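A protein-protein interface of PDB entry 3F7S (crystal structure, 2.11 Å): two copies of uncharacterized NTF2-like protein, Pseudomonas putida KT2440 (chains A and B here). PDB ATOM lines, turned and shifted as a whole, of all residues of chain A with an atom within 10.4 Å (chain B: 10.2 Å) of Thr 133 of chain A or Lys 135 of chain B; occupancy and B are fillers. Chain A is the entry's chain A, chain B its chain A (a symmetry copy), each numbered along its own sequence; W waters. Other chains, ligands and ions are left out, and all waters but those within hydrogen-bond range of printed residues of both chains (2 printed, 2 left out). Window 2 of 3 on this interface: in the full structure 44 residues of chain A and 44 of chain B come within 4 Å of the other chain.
The backbone NH of Phe 129 of chain B sits at hydrogen-bond distance from the backbone carbonyl oxygen of Ala 42 of chain A, at 3.0 Å.
The backbone carbonyl oxygen of Phe 129 of chain B is in hydrogen-bond range of the backbone NH of Gln 44 of chain A (3.2 Å).
The backbone NH (N) of Phe 129 of chain A lies within hydrogen-bond range of the backbone carbonyl oxygen (O) of Ala 42 of chain B (3.0 Å).
The backbone carbonyl oxygen (O) of Phe 129 of chain A sits at hydrogen-bond distance from the backbone NH (N) of Gln 44 of chain B, at 3.2 Å.
O of Gln 134 of chain A is in hydrogen-bond range of N of Ala 136 of chain B (2.9 Å).
The backbone NH (N) of Ala 136 of chain A is in hydrogen-bond range of the backbone carbonyl oxygen (O) of Gln 134 of chain B (2.9 Å).
O of Pro 128 of chain A lies within hydrogen-bond range of N of Leu 137 of chain A (2.8 Å).
OD2 of Asp 130 of chain A is in hydrogen-bond range of N of Thr 133 of chain A, at 2.8 Å.
O of Lys 135 of chain A is in hydrogen-bond range of N of Asp 130 of chain A (2.9 Å).
OG1 of Thr 133 of chain A lies close to N of Lys 135 of chain A.
The side-chain carboxylate (OD2) of Asp 130 of chain B is in hydrogen-bond range of the backbone NH (N) of Thr 133 of chain B (2.8 Å).
OG1 of Thr 133 of chain B sits close to N of Lys 135 of chain B (3.3 Å).
Among the printed residues, merely in contact across the chains: Ile 43 of chain A with Phe 129 of chain B (3.3 Å), Phe 129 of chain A with Ile 43 of chain B (3.3 Å), Phe 129 of chain A with Phe 138 of chain B (3.3 Å), Phe 138 of chain A with Phe 129 of chain B (3.3 Å), Pro 128 of chain A with Ala 42 of chain B (3.4 Å), Ala 42 of chain A with Pro 128 of chain B (3.4 Å), Thr 133 of chain A with Lys 135 of chain B (3.4 Å), Lys 135 of chain A with Thr 133 of chain B (3.4 Å), Gln 134 of chain A with Lys 135 of chain B (3.4 Å), Lys 135 of chain A with Gln 134 of chain B (3.4 Å), Ala 45 of chain A with Pro 128 of chain B (3.5 Å), Met 131 of chain A with Ile 43 of chain B (3.6 Å), Ile 43 of chain A with Met 131 of chain B (3.6 Å), Phe 138 of chain A with Gln 134 of chain B (3.7 Å), Gln 134 of chain A with Phe 138 of chain B (3.7 Å), Ala 136 of chain A with Phe 129 of chain B (3.8 Å), Phe 129 of chain A with Ala 136 of chain B (3.8 Å), Gln 44 of chain A with Leu 140 of chain B (3.9 Å), Ala 45 of chain A with Leu 140 of chain B (3.9 Å), Phe 129 of chain A with Ala 127 of chain B (3.9 Å) and Ala 127 of chain A with Phe 129 of chain B (3.9 Å).
Thr 133 of chain A touches just one residue of chain B: Lys 135 (3.4 Å).
Of chain A, only Thr 133 and Gln 134 come within 4 Å of Lys 135 of chain B.
No residue of chain B comes within 4 Å of Asp 130 of chain A.
No residue of chain B comes within 4 Å of Glu 132 of chain A.
Of chain B, only Lys 135, Ala 136 and Phe 138 come within 4 Å of Gln 134 of chain A.
Lys 135 of chain A touches two residues of chain B.
No residue of chain A comes within 4 Å of Asp 130 of chain B.
Of chain A, only Lys 135 (3.4 Å) comes within 4 Å of Thr 133 of chain B.
Ala 136 of chain B touches just these residues of chain A: Phe 129 (3.8 Å) and Gln 134 (2.9 Å).
Printed residues of chain B within 4 Å of Ile 43 of chain A: Phe 129 (3.3 Å) and Met 131 (3.6 Å).
Of the printed residues of chain B, Ala 45 of chain A touches Pro 128 (3.5 Å) and Leu 140 (3.9 Å).
Printed residues of chain A within 4 Å of Leu 140 of chain B: Gln 44 (3.9 Å) and Ala 45 (3.9 Å).
Glu 132 of chain B touches none of the printed residues of chain A.
Asp 139 of chain B touches none of the printed residues of chain A.
The nearest residue of chain A that does not touch Lys 135 of chain B is Lys 135 of chain A (4.3 Å).
Printed residues of chain B that touch a printed residue of chain A: Ala 42, Ile 43, Gln 44, Ala 127, Pro 128, Phe 129, Met 131, Thr 133, Gln 134, Lys 135, Ala 136, Phe 138 and Leu 140.
Hydrophobic or aromatic side chains of chain B that line the printed part of chain A: Ile 43, Ala 127, Pro 128, Phe 129, Met 131, Ala 136, Phe 138 and Leu 140.
Of the 17 printed residues of chain A, 13 touch a printed residue of chain B.
Among the printed residues, 27 pairs touch across the chains.
Among the printed residues, no Asp or Glu carboxylate lies within 4 Å of a Lys or Arg side-chain nitrogen of the other chain.
Ala 42 of chain A touches Pro 128 of chain B, and with the chains exchanged Pro 128 of chain A touches Ala 42 of chain B.
Ala 42 of chain A touches Phe 129 of chain B, and with the chains exchanged Phe 129 of chain A touches Ala 42 of chain B.
Ile 43 of chain A touches Phe 129 of chain B, and with the chains exchanged Phe 129 of chain A touches Ile 43 of chain B.
Gln 134 of chain A touches Phe 138 of chain B, and with the chains exchanged Phe 138 of chain A touches Gln 134 of chain B.
Positions printed for both chains: 42, 43, 44, 127, 128, 129, 130, 131, 132, 133, 134, 135, 136, 137, 138 and 139.
Of the 27 pairs that touch across the chains among the printed residues, 24 have their exchanged pair printed and touching as well.
Water W2 lies within hydrogen-bond range of O of Ala 42 of chain B (2.9 Å), O of Ala 127 of chain A (2.9 Å) and N of Ala 127 of chain B (3.0 Å).
Water W1 lies within hydrogen-bond range of the backbone carbonyl oxygen of Ala 42 of chain A, the backbone carbonyl oxygen of Ala 127 of chain B and the backbone NH of Ala 127 of chain A.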
ATOM      1  N   ALA A  42     -21.243 -28.792 -22.463  1.00  0.00           N
ATOM      2  CA  ALA A  42     -21.561 -27.928 -21.328  1.00  0.00           C
ATOM      3  C   ALA A  42     -20.980 -28.448 -20.030  1.00  0.00           C
ATOM      4  O   ALA A  42     -20.884 -27.682 -19.058  1.00  0.00           O
ATOM      5  CB  ALA A  42     -23.085 -27.768 -21.203  1.00  0.00           C
ATOM      6  N   ILE A  43     -20.621 -29.743 -20.014  1.00  0.00           N
ATOM      7  CA  ILE A  43     -20.161 -30.405 -18.797  1.00  0.00           C
ATOM      8  C   ILE A  43     -18.868 -31.197 -18.946  1.00  0.00           C
ATOM      9  O   ILE A  43     -18.494 -31.586 -20.055  1.00  0.00           O
ATOM     10  CB  ILE A  43     -21.245 -31.395 -18.264  1.00  0.00           C
ATOM     11  CG1 ILE A  43     -21.556 -32.495 -19.285  1.00  0.00           C
ATOM     12  CG2 ILE A  43     -22.559 -30.651 -17.897  1.00  0.00           C
ATOM     13  CD1 ILE A  43     -22.512 -33.611 -18.698  1.00  0.00           C
ATOM     14  N   GLN A  44     -18.205 -31.412 -17.809  1.00  0.00           N
ATOM     15  CA  GLN A  44     -17.257 -32.537 -17.587  1.00  0.00           C
ATOM     16  C   GLN A  44     -15.828 -32.402 -18.163  1.00  0.00           C
ATOM     17  O   GLN A  44     -14.841 -32.706 -17.474  1.00  0.00           O
ATOM     18  CB  GLN A  44     -17.893 -33.819 -18.085  1.00  0.00           C
ATOM     19  CG  GLN A  44     -17.080 -35.109 -17.914  1.00  0.00           C
ATOM     20  CD  GLN A  44     -17.702 -36.261 -18.727  1.00  0.00           C
ATOM     21  OE1 GLN A  44     -18.896 -36.540 -18.600  1.00  0.00           O
ATOM     22  NE2 GLN A  44     -16.900 -36.902 -19.585  1.00  0.00           N
ATOM     23  N   ALA A  45     -15.722 -31.954 -19.412  1.00  0.00           N
ATOM     24  CA  ALA A  45     -14.441 -31.853 -20.081  1.00  0.00           C
ATOM     25  C   ALA A  45     -14.377 -30.557 -20.901  1.00  0.00           C
ATOM     26  O   ALA A  45     -15.393 -29.969 -21.269  1.00  0.00           O
ATOM     27  CB  ALA A  45     -14.220 -33.086 -20.957  1.00  0.00           C
ATOM     28  N   ALA A 127     -23.617 -23.244 -20.156  1.00  0.00           N
ATOM     29  CA  ALA A 127     -24.279 -22.319 -19.251  1.00  0.00           C
ATOM     30  C   ALA A 127     -23.279 -21.228 -18.797  1.00  0.00           C
ATOM     31  O   ALA A 127     -22.083 -21.504 -18.573  1.00  0.00           O
ATOM     32  CB  ALA A 127     -24.864 -23.067 -17.960  1.00  0.00           C
ATOM     33  N   PRO A 128     -23.777 -19.991 -18.609  1.00  0.00           N
ATOM     34  CA  PRO A 128     -22.942 -18.940 -18.027  1.00  0.00           C
ATOM     35  C   PRO A 128     -22.721 -19.246 -16.563  1.00  0.00           C
ATOM     36  O   PRO A 128     -23.532 -19.948 -15.975  1.00  0.00           O
ATOM     37  CB  PRO A 128     -23.804 -17.669 -18.172  1.00  0.00           C
ATOM     38  CG  PRO A 128     -25.202 -18.132 -18.322  1.00  0.00           C
ATOM     39  CD  PRO A 128     -25.178 -19.565 -18.803  1.00  0.00           C
ATOM     40  N   PHE A 129     -21.666 -18.716 -15.963  1.00  0.00           N
ATOM     41  CA  PHE A 129     -21.499 -18.862 -14.507  1.00  0.00           C
ATOM     42  C   PHE A 129     -21.391 -17.518 -13.786  1.00  0.00           C
ATOM     43  O   PHE A 129     -21.203 -16.471 -14.396  1.00  0.00           O
ATOM     44  CB  PHE A 129     -20.306 -19.764 -14.156  1.00  0.00           C
ATOM     45  CG  PHE A 129     -18.994 -19.218 -14.580  1.00  0.00           C
ATOM     46  CD1 PHE A 129     -18.303 -18.329 -13.760  1.00  0.00           C
ATOM     47  CD2 PHE A 129     -18.438 -19.593 -15.787  1.00  0.00           C
ATOM     48  CE1 PHE A 129     -17.086 -17.801 -14.148  1.00  0.00           C
ATOM     49  CE2 PHE A 129     -17.228 -19.068 -16.184  1.00  0.00           C
ATOM     50  CZ  PHE A 129     -16.552 -18.177 -15.370  1.00  0.00           C
ATOM     51  N   ASP A 130     -21.497 -17.568 -12.470  1.00  0.00           N
ATOM     52  CA  ASP A 130     -21.318 -16.373 -11.616  1.00  0.00           C
ATOM     53  C   ASP A 130     -19.848 -16.214 -11.210  1.00  0.00           C
ATOM     54  O   ASP A 130     -19.234 -17.131 -10.707  1.00  0.00           O
ATOM     55  CB  ASP A 130     -22.189 -16.521 -10.383  1.00  0.00           C
ATOM     56  CG  ASP A 130     -22.083 -15.323  -9.417  1.00  0.00           C
ATOM     57  OD1 ASP A 130     -22.267 -14.165  -9.828  1.00  0.00           O
ATOM     58  OD2 ASP A 130     -21.841 -15.554  -8.230  1.00  0.00           O
ATOM     59  N   MET A 131     -19.275 -15.055 -11.456  1.00  0.00           N
ATOM     60  CA  MET A 131     -17.924 -14.772 -11.008  1.00  0.00           C
ATOM     61  C   MET A 131     -17.677 -15.113  -9.539  1.00  0.00           C
ATOM     62  O   MET A 131     -16.688 -15.737  -9.204  1.00  0.00           O
ATOM     63  CB  MET A 131     -17.654 -13.286 -11.167  1.00  0.00           C
ATOM     64  CG  MET A 131     -17.604 -12.786 -12.601  1.00  0.00           C
ATOM     65  SD  MET A 131     -15.886 -13.195 -13.443  1.00  0.00           S
ATOM     66  CE  MET A 131     -15.531 -11.339 -14.099  1.00  0.00           C
ATOM     67  N   GLU A 132     -18.579 -14.699  -8.662  1.00  0.00           N
ATOM     68  CA  GLU A 132     -18.307 -14.752  -7.231  1.00  0.00           C
ATOM     69  C   GLU A 132     -18.497 -16.155  -6.705  1.00  0.00           C
ATOM     70  O   GLU A 132     -17.615 -16.688  -6.037  1.00  0.00           O
ATOM     71  CB  GLU A 132     -19.206 -13.785  -6.455  1.00  0.00           C
ATOM     72  N   THR A 133     -19.644 -16.748  -6.995  1.00  0.00           N
ATOM     73  CA  THR A 133     -19.926 -18.111  -6.576  1.00  0.00           C
ATOM     74  C   THR A 133     -19.270 -19.196  -7.472  1.00  0.00           C
ATOM     75  O   THR A 133     -19.222 -20.353  -7.087  1.00  0.00           O
ATOM     76  CB  THR A 133     -21.467 -18.375  -6.515  1.00  0.00           C
ATOM     77  OG1 THR A 133     -22.020 -18.393  -7.831  1.00  0.00           O
ATOM     78  CG2 THR A 133     -22.204 -17.289  -5.673  1.00  0.00           C
ATOM     79  N   GLN A 134     -18.795 -18.815  -8.660  1.00  0.00           N
ATOM     80  CA  GLN A 134     -18.384 -19.771  -9.715  1.00  0.00           C
ATOM     81  C   GLN A 134     -19.367 -20.922  -9.979  1.00  0.00           C
ATOM     82  O   GLN A 134     -18.979 -21.991 -10.422  1.00  0.00           O
ATOM     83  CB  GLN A 134     -16.997 -20.312  -9.402  1.00  0.00           C
ATOM     84  CG  GLN A 134     -16.002 -19.186  -9.150  1.00  0.00           C
ATOM     85  CD  GLN A 134     -14.550 -19.642  -9.152  1.00  0.00           C
ATOM     86  OE1 GLN A 134     -13.664 -18.880  -9.542  1.00  0.00           O
ATOM     87  NE2 GLN A 134     -14.297 -20.883  -8.713  1.00  0.00           N
ATOM     88  N   LYS A 135     -20.645 -20.677  -9.730  1.00  0.00           N
ATOM     89  CA  LYS A 135     -21.665 -21.657  -9.999  1.00  0.00           C
ATOM     90  C   LYS A 135     -22.322 -21.338 -11.344  1.00  0.00           C
ATOM     91  O   LYS A 135     -22.421 -20.167 -11.716  1.00  0.00           O
ATOM     92  CB  LYS A 135     -22.692 -21.661  -8.867  1.00  0.00           C
ATOM     93  CG  LYS A 135     -22.109 -22.170  -7.547  1.00  0.00           C
ATOM     94  CD  LYS A 135     -23.162 -22.725  -6.602  1.00  0.00           C
ATOM     95  CE  LYS A 135     -23.221 -24.253  -6.604  1.00  0.00           C
ATOM     96  NZ  LYS A 135     -23.886 -24.784  -5.347  1.00  0.00           N
ATOM     97  N   ALA A 136     -22.734 -22.395 -12.061  1.00  0.00           N
ATOM     98  CA  ALA A 136     -23.421 -22.286 -13.359  1.00  0.00           C
ATOM     99  C   ALA A 136     -24.778 -21.658 -13.093  1.00  0.00           C
ATOM    100  O   ALA A 136     -25.422 -22.005 -12.124  1.00  0.00           O
ATOM    101  CB  ALA A 136     -23.594 -23.680 -14.014  1.00  0.00           C
ATOM    102  N   LEU A 137     -25.206 -20.733 -13.938  1.00  0.00           N
ATOM    103  CA  LEU A 137     -26.487 -20.077 -13.754  1.00  0.00           C
ATOM    104  C   LEU A 137     -27.498 -20.732 -14.651  1.00  0.00           C
ATOM    105  O   LEU A 137     -27.363 -20.706 -15.889  1.00  0.00           O
ATOM    106  CB  LEU A 137     -26.379 -18.588 -14.067  1.00  0.00           C
ATOM    107  CG  LEU A 137     -25.348 -17.833 -13.209  1.00  0.00           C
ATOM    108  CD1 LEU A 137     -24.894 -16.499 -13.858  1.00  0.00           C
ATOM    109  CD2 LEU A 137     -25.899 -17.586 -11.838  1.00  0.00           C
ATOM    110  N   PHE A 138     -28.509 -21.324 -14.021  1.00  0.00           N
ATOM    111  CA  PHE A 138     -29.529 -22.087 -14.717  1.00  0.00           C
ATOM    112  C   PHE A 138     -30.926 -21.452 -14.789  1.00  0.00           C
ATOM    113  O   PHE A 138     -31.752 -21.928 -15.559  1.00  0.00           O
ATOM    114  CB  PHE A 138     -29.638 -23.477 -14.080  1.00  0.00           C
ATOM    115  CG  PHE A 138     -28.401 -24.308 -14.248  1.00  0.00           C
ATOM    116  CD1 PHE A 138     -28.050 -24.800 -15.489  1.00  0.00           C
ATOM    117  CD2 PHE A 138     -27.583 -24.586 -13.162  1.00  0.00           C
ATOM    118  CE1 PHE A 138     -26.911 -25.556 -15.630  1.00  0.00           C
ATOM    119  CE2 PHE A 138     -26.442 -25.334 -13.307  1.00  0.00           C
ATOM    120  CZ  PHE A 138     -26.108 -25.817 -14.524  1.00  0.00           C
ATOM    121  N   ASP A 139     -31.187 -20.379 -14.032  1.00  0.00           N
ATOM    122  CA  ASP A 139     -32.520 -19.778 -13.995  1.00  0.00           C
ATOM    123  C   ASP A 139     -32.673 -18.476 -14.811  1.00  0.00           C
ATOM    124  O   ASP A 139     -33.603 -17.704 -14.584  1.00  0.00           O
ATOM    125  CB  ASP A 139     -32.945 -19.571 -12.528  1.00  0.00           C
ATOM    126  CG  ASP A 139     -32.396 -18.279 -11.919  1.00  0.00           C
ATOM    127  OD1 ASP A 139     -31.238 -17.925 -12.254  1.00  0.00           O
ATOM    128  OD2 ASP A 139     -33.118 -17.627 -11.099  1.00  0.00           O
ATOM    129  N   ALA B  42     -19.223 -15.940 -21.122  1.00  0.00           N
ATOM    130  CA  ALA B  42     -18.965 -17.014 -20.165  1.00  0.00           C
ATOM    131  C   ALA B  42     -19.622 -16.757 -18.824  1.00  0.00           C
ATOM    132  O   ALA B  42     -19.769 -17.699 -18.030  1.00  0.00           O
ATOM    133  CB  ALA B  42     -17.450 -17.203 -19.987  1.00  0.00           C
ATOM    134  N   ILE B  43     -19.989 -15.489 -18.573  1.00  0.00           N
ATOM    135  CA  ILE B  43     -20.520 -15.077 -17.278  1.00  0.00           C
ATOM    136  C   ILE B  43     -21.808 -14.264 -17.340  1.00  0.00           C
ATOM    137  O   ILE B  43     -22.120 -13.662 -18.370  1.00  0.00           O
ATOM    138  CB  ILE B  43     -19.474 -14.219 -16.499  1.00  0.00           C
ATOM    139  CG1 ILE B  43     -19.112 -12.940 -17.263  1.00  0.00           C
ATOM    140  CG2 ILE B  43     -18.179 -15.027 -16.212  1.00  0.00           C
ATOM    141  CD1 ILE B  43     -18.197 -11.967 -16.414  1.00  0.00           C
ATOM    142  N   GLN B  44     -22.535 -14.274 -16.222  1.00  0.00           N
ATOM    143  CA  GLN B  44     -23.500 -13.210 -15.838  1.00  0.00           C
ATOM    144  C   GLN B  44     -24.894 -13.220 -16.509  1.00  0.00           C
ATOM    145  O   GLN B  44     -25.920 -13.052 -15.830  1.00  0.00           O
ATOM    146  CB  GLN B  44     -22.844 -11.858 -16.035  1.00  0.00           C
ATOM    147  CG  GLN B  44     -23.673 -10.623 -15.660  1.00  0.00           C
ATOM    148  CD  GLN B  44     -23.013  -9.336 -16.193  1.00  0.00           C
ATOM    149  OE1 GLN B  44     -21.829  -9.095 -15.946  1.00  0.00           O
ATOM    150  NE2 GLN B  44     -23.769  -8.534 -16.951  1.00  0.00           N
ATOM    151  N   ALA B 127     -16.952 -21.849 -19.825  1.00  0.00           N
ATOM    152  CA  ALA B 127     -16.338 -22.937 -19.085  1.00  0.00           C
ATOM    153  C   ALA B 127     -17.356 -24.091 -18.913  1.00  0.00           C
ATOM    154  O   ALA B 127     -18.564 -23.858 -18.707  1.00  0.00           O
ATOM    155  CB  ALA B 127     -15.832 -22.462 -17.641  1.00  0.00           C
ATOM    156  N   PRO B 128     -16.862 -25.343 -18.945  1.00  0.00           N
ATOM    157  CA  PRO B 128     -17.723 -26.484 -18.630  1.00  0.00           C
ATOM    158  C   PRO B 128     -18.028 -26.472 -17.150  1.00  0.00           C
ATOM    159  O   PRO B 128     -17.256 -25.904 -16.389  1.00  0.00           O
ATOM    160  CB  PRO B 128     -16.847 -27.706 -18.974  1.00  0.00           C
ATOM    161  CG  PRO B 128     -15.446 -27.231 -18.950  1.00  0.00           C
ATOM    162  CD  PRO B 128     -15.450 -25.731 -19.140  1.00  0.00           C
ATOM    163  N   PHE B 129     -19.112 -27.104 -16.726  1.00  0.00           N
ATOM    164  CA  PHE B 129     -19.363 -27.248 -15.283  1.00  0.00           C
ATOM    165  C   PHE B 129     -19.504 -28.707 -14.849  1.00  0.00           C
ATOM    166  O   PHE B 129     -19.652 -29.611 -15.663  1.00  0.00           O
ATOM    167  CB  PHE B 129     -20.579 -26.426 -14.828  1.00  0.00           C
ATOM    168  CG  PHE B 129     -21.861 -26.870 -15.426  1.00  0.00           C
ATOM    169  CD1 PHE B 129     -22.593 -27.899 -14.838  1.00  0.00           C
ATOM    170  CD2 PHE B 129     -22.351 -26.260 -16.565  1.00  0.00           C
ATOM    171  CE1 PHE B 129     -23.783 -28.333 -15.391  1.00  0.00           C
ATOM    172  CE2 PHE B 129     -23.533 -26.690 -17.125  1.00  0.00           C
ATOM    173  CZ  PHE B 129     -24.249 -27.720 -16.544  1.00  0.00           C
ATOM    174  N   ASP B 130     -19.473 -28.919 -13.545  1.00  0.00           N
ATOM    175  CA  ASP B 130     -19.693 -30.257 -12.955  1.00  0.00           C
ATOM    176  C   ASP B 130     -21.184 -30.484 -12.672  1.00  0.00           C
ATOM    177  O   ASP B 130     -21.830 -29.681 -12.034  1.00  0.00           O
ATOM    178  CB  ASP B 130     -18.895 -30.360 -11.669  1.00  0.00           C
ATOM    179  CG  ASP B 130     -19.049 -31.725 -10.967  1.00  0.00           C
ATOM    180  OD1 ASP B 130     -18.835 -32.780 -11.588  1.00  0.00           O
ATOM    181  OD2 ASP B 130     -19.359 -31.731  -9.773  1.00  0.00           O
ATOM    182  N   MET B 131     -21.735 -31.569 -13.174  1.00  0.00           N
ATOM    183  CA  MET B 131     -23.108 -31.927 -12.869  1.00  0.00           C
ATOM    184  C   MET B 131     -23.440 -31.882 -11.378  1.00  0.00           C
ATOM    185  O   MET B 131     -24.450 -31.331 -10.983  1.00  0.00           O
ATOM    186  CB  MET B 131     -23.360 -33.351 -13.334  1.00  0.00           C
ATOM    187  CG  MET B 131     -23.325 -33.558 -14.838  1.00  0.00           C
ATOM    188  SD  MET B 131     -24.995 -32.981 -15.679  1.00  0.00           S
ATOM    189  CE  MET B 131     -25.302 -34.669 -16.708  1.00  0.00           C
ATOM    190  N   GLU B 132     -22.586 -32.466 -10.550  1.00  0.00           N
ATOM    191  CA  GLU B 132     -22.939 -32.695  -9.155  1.00  0.00           C
ATOM    192  C   GLU B 132     -22.788 -31.425  -8.352  1.00  0.00           C
ATOM    193  O   GLU B 132     -23.710 -31.029  -7.644  1.00  0.00           O
ATOM    194  CB  GLU B 132     -22.080 -33.801  -8.535  1.00  0.00           C
ATOM    195  N   THR B 133     -21.629 -30.793  -8.454  1.00  0.00           N
ATOM    196  CA  THR B 133     -21.379 -29.540  -7.758  1.00  0.00           C
ATOM    197  C   THR B 133     -21.989 -28.297  -8.458  1.00  0.00           C
ATOM    198  O   THR B 133     -22.066 -27.238  -7.856  1.00  0.00           O
ATOM    199  CB  THR B 133     -19.846 -29.303  -7.559  1.00  0.00           C
ATOM    200  OG1 THR B 133     -19.219 -29.028  -8.811  1.00  0.00           O
ATOM    201  CG2 THR B 133     -19.151 -30.538  -6.907  1.00  0.00           C
ATOM    202  N   GLN B 134     -22.394 -28.433  -9.723  1.00  0.00           N
ATOM    203  CA  GLN B 134     -22.750 -27.285 -10.590  1.00  0.00           C
ATOM    204  C   GLN B 134     -21.760 -26.110 -10.565  1.00  0.00           C
ATOM    205  O   GLN B 134     -22.129 -24.973 -10.810  1.00  0.00           O
ATOM    206  CB  GLN B 134     -24.156 -26.808 -10.256  1.00  0.00           C
ATOM    207  CG  GLN B 134     -25.157 -27.956 -10.288  1.00  0.00           C
ATOM    208  CD  GLN B 134     -26.609 -27.501 -10.282  1.00  0.00           C
ATOM    209  OE1 GLN B 134     -27.467 -28.166 -10.864  1.00  0.00           O
ATOM    210  NE2 GLN B 134     -26.893 -26.369  -9.622  1.00  0.00           N
ATOM    211  N   LYS B 135     -20.497 -26.407 -10.298  1.00  0.00           N
ATOM    212  CA  LYS B 135     -19.469 -25.399 -10.310  1.00  0.00           C
ATOM    213  C   LYS B 135     -18.734 -25.449 -11.652  1.00  0.00           C
ATOM    214  O   LYS B 135     -18.608 -26.524 -12.241  1.00  0.00           O
ATOM    215  CB  LYS B 135     -18.508 -25.624  -9.142  1.00  0.00           C
ATOM    216  CG  LYS B 135     -19.168 -25.383  -7.784  1.00  0.00           C
ATOM    217  CD  LYS B 135     -18.173 -25.031  -6.689  1.00  0.00           C
ATOM    218  CE  LYS B 135     -18.123 -23.533  -6.386  1.00  0.00           C
ATOM    219  NZ  LYS B 135     -17.534 -23.264  -5.013  1.00  0.00           N
ATOM    220  N   ALA B 136     -18.289 -24.274 -12.121  1.00  0.00           N
ATOM    221  CA  ALA B 136     -17.529 -24.128 -13.374  1.00  0.00           C
ATOM    222  C   ALA B 136     -16.185 -24.804 -13.161  1.00  0.00           C
ATOM    223  O   ALA B 136     -15.600 -24.659 -12.107  1.00  0.00           O
ATOM    224  CB  ALA B 136     -17.327 -22.634 -13.730  1.00  0.00           C
ATOM    225  N   LEU B 137     -15.705 -25.547 -14.146  1.00  0.00           N
ATOM    226  CA  LEU B 137     -14.432 -26.234 -14.022  1.00  0.00           C
ATOM    227  C   LEU B 137     -13.376 -25.420 -14.713  1.00  0.00           C
ATOM    228  O   LEU B 137     -13.441 -25.200 -15.938  1.00  0.00           O
ATOM    229  CB  LEU B 137     -14.514 -27.631 -14.630  1.00  0.00           C
ATOM    230  CG  LEU B 137     -15.588 -28.534 -13.997  1.00  0.00           C
ATOM    231  CD1 LEU B 137     -15.997 -29.711 -14.922  1.00  0.00           C
ATOM    232  CD2 LEU B 137     -15.115 -29.051 -12.673  1.00  0.00           C
ATOM    233  N   PHE B 138     -12.406 -24.969 -13.923  1.00  0.00           N
ATOM    234  CA  PHE B 138     -11.353 -24.090 -14.396  1.00  0.00           C
ATOM    235  C   PHE B 138      -9.950 -24.706 -14.512  1.00  0.00           C
ATOM    236  O   PHE B 138      -9.084 -24.092 -15.125  1.00  0.00           O
ATOM    237  CB  PHE B 138     -11.288 -22.854 -13.492  1.00  0.00           C
ATOM    238  CG  PHE B 138     -12.518 -21.999 -13.562  1.00  0.00           C
ATOM    239  CD1 PHE B 138     -12.800 -21.270 -14.699  1.00  0.00           C
ATOM    240  CD2 PHE B 138     -13.398 -21.936 -12.491  1.00  0.00           C
ATOM    241  CE1 PHE B 138     -13.934 -20.494 -14.752  1.00  0.00           C
ATOM    242  CE2 PHE B 138     -14.533 -21.168 -12.550  1.00  0.00           C
ATOM    243  CZ  PHE B 138     -14.800 -20.452 -13.665  1.00  0.00           C
ATOM    244  N   ASP B 139      -9.727 -25.909 -13.968  1.00  0.00           N
ATOM    245  CA  ASP B 139      -8.394 -26.513 -13.975  1.00  0.00           C
ATOM    246  C   ASP B 139      -8.188 -27.629 -15.022  1.00  0.00           C
ATOM    247  O   ASP B 139      -7.267 -28.436 -14.899  1.00  0.00           O
ATOM    248  CB  ASP B 139      -8.052 -27.008 -12.556  1.00  0.00           C
ATOM    249  CG  ASP B 139      -8.627 -28.392 -12.246  1.00  0.00           C
ATOM    250  OD1 ASP B 139      -9.762 -28.666 -12.710  1.00  0.00           O
ATOM    251  OD2 ASP B 139      -7.950 -29.197 -11.531  1.00  0.00           O
ATOM    252  N   LEU B 140      -9.010 -27.671 -16.059  1.00  0.00           N
ATOM    253  CA  LEU B 140      -8.944 -28.761 -17.038  1.00  0.00           C
ATOM    254  C   LEU B 140      -7.869 -28.551 -18.125  1.00  0.00           C
ATOM    255  O   LEU B 140      -7.590 -27.424 -18.525  1.00  0.00           O
ATOM    256  CB  LEU B 140     -10.313 -28.954 -17.687  1.00  0.00           C
ATOM    257  CG  LEU B 140     -11.496 -29.125 -16.734  1.00  0.00           C
ATOM    258  CD1 LEU B 140     -12.735 -29.429 -17.551  1.00  0.00           C
ATOM    259  CD2 LEU B 140     -11.266 -30.203 -15.638  1.00  0.00           C
HETATM  260  O   HOH W   1     -21.117 -24.869 -19.537  1.00  0.00           O
HETATM  261  O   HOH W   2     -19.493 -20.363 -19.041  1.00  0.00           O
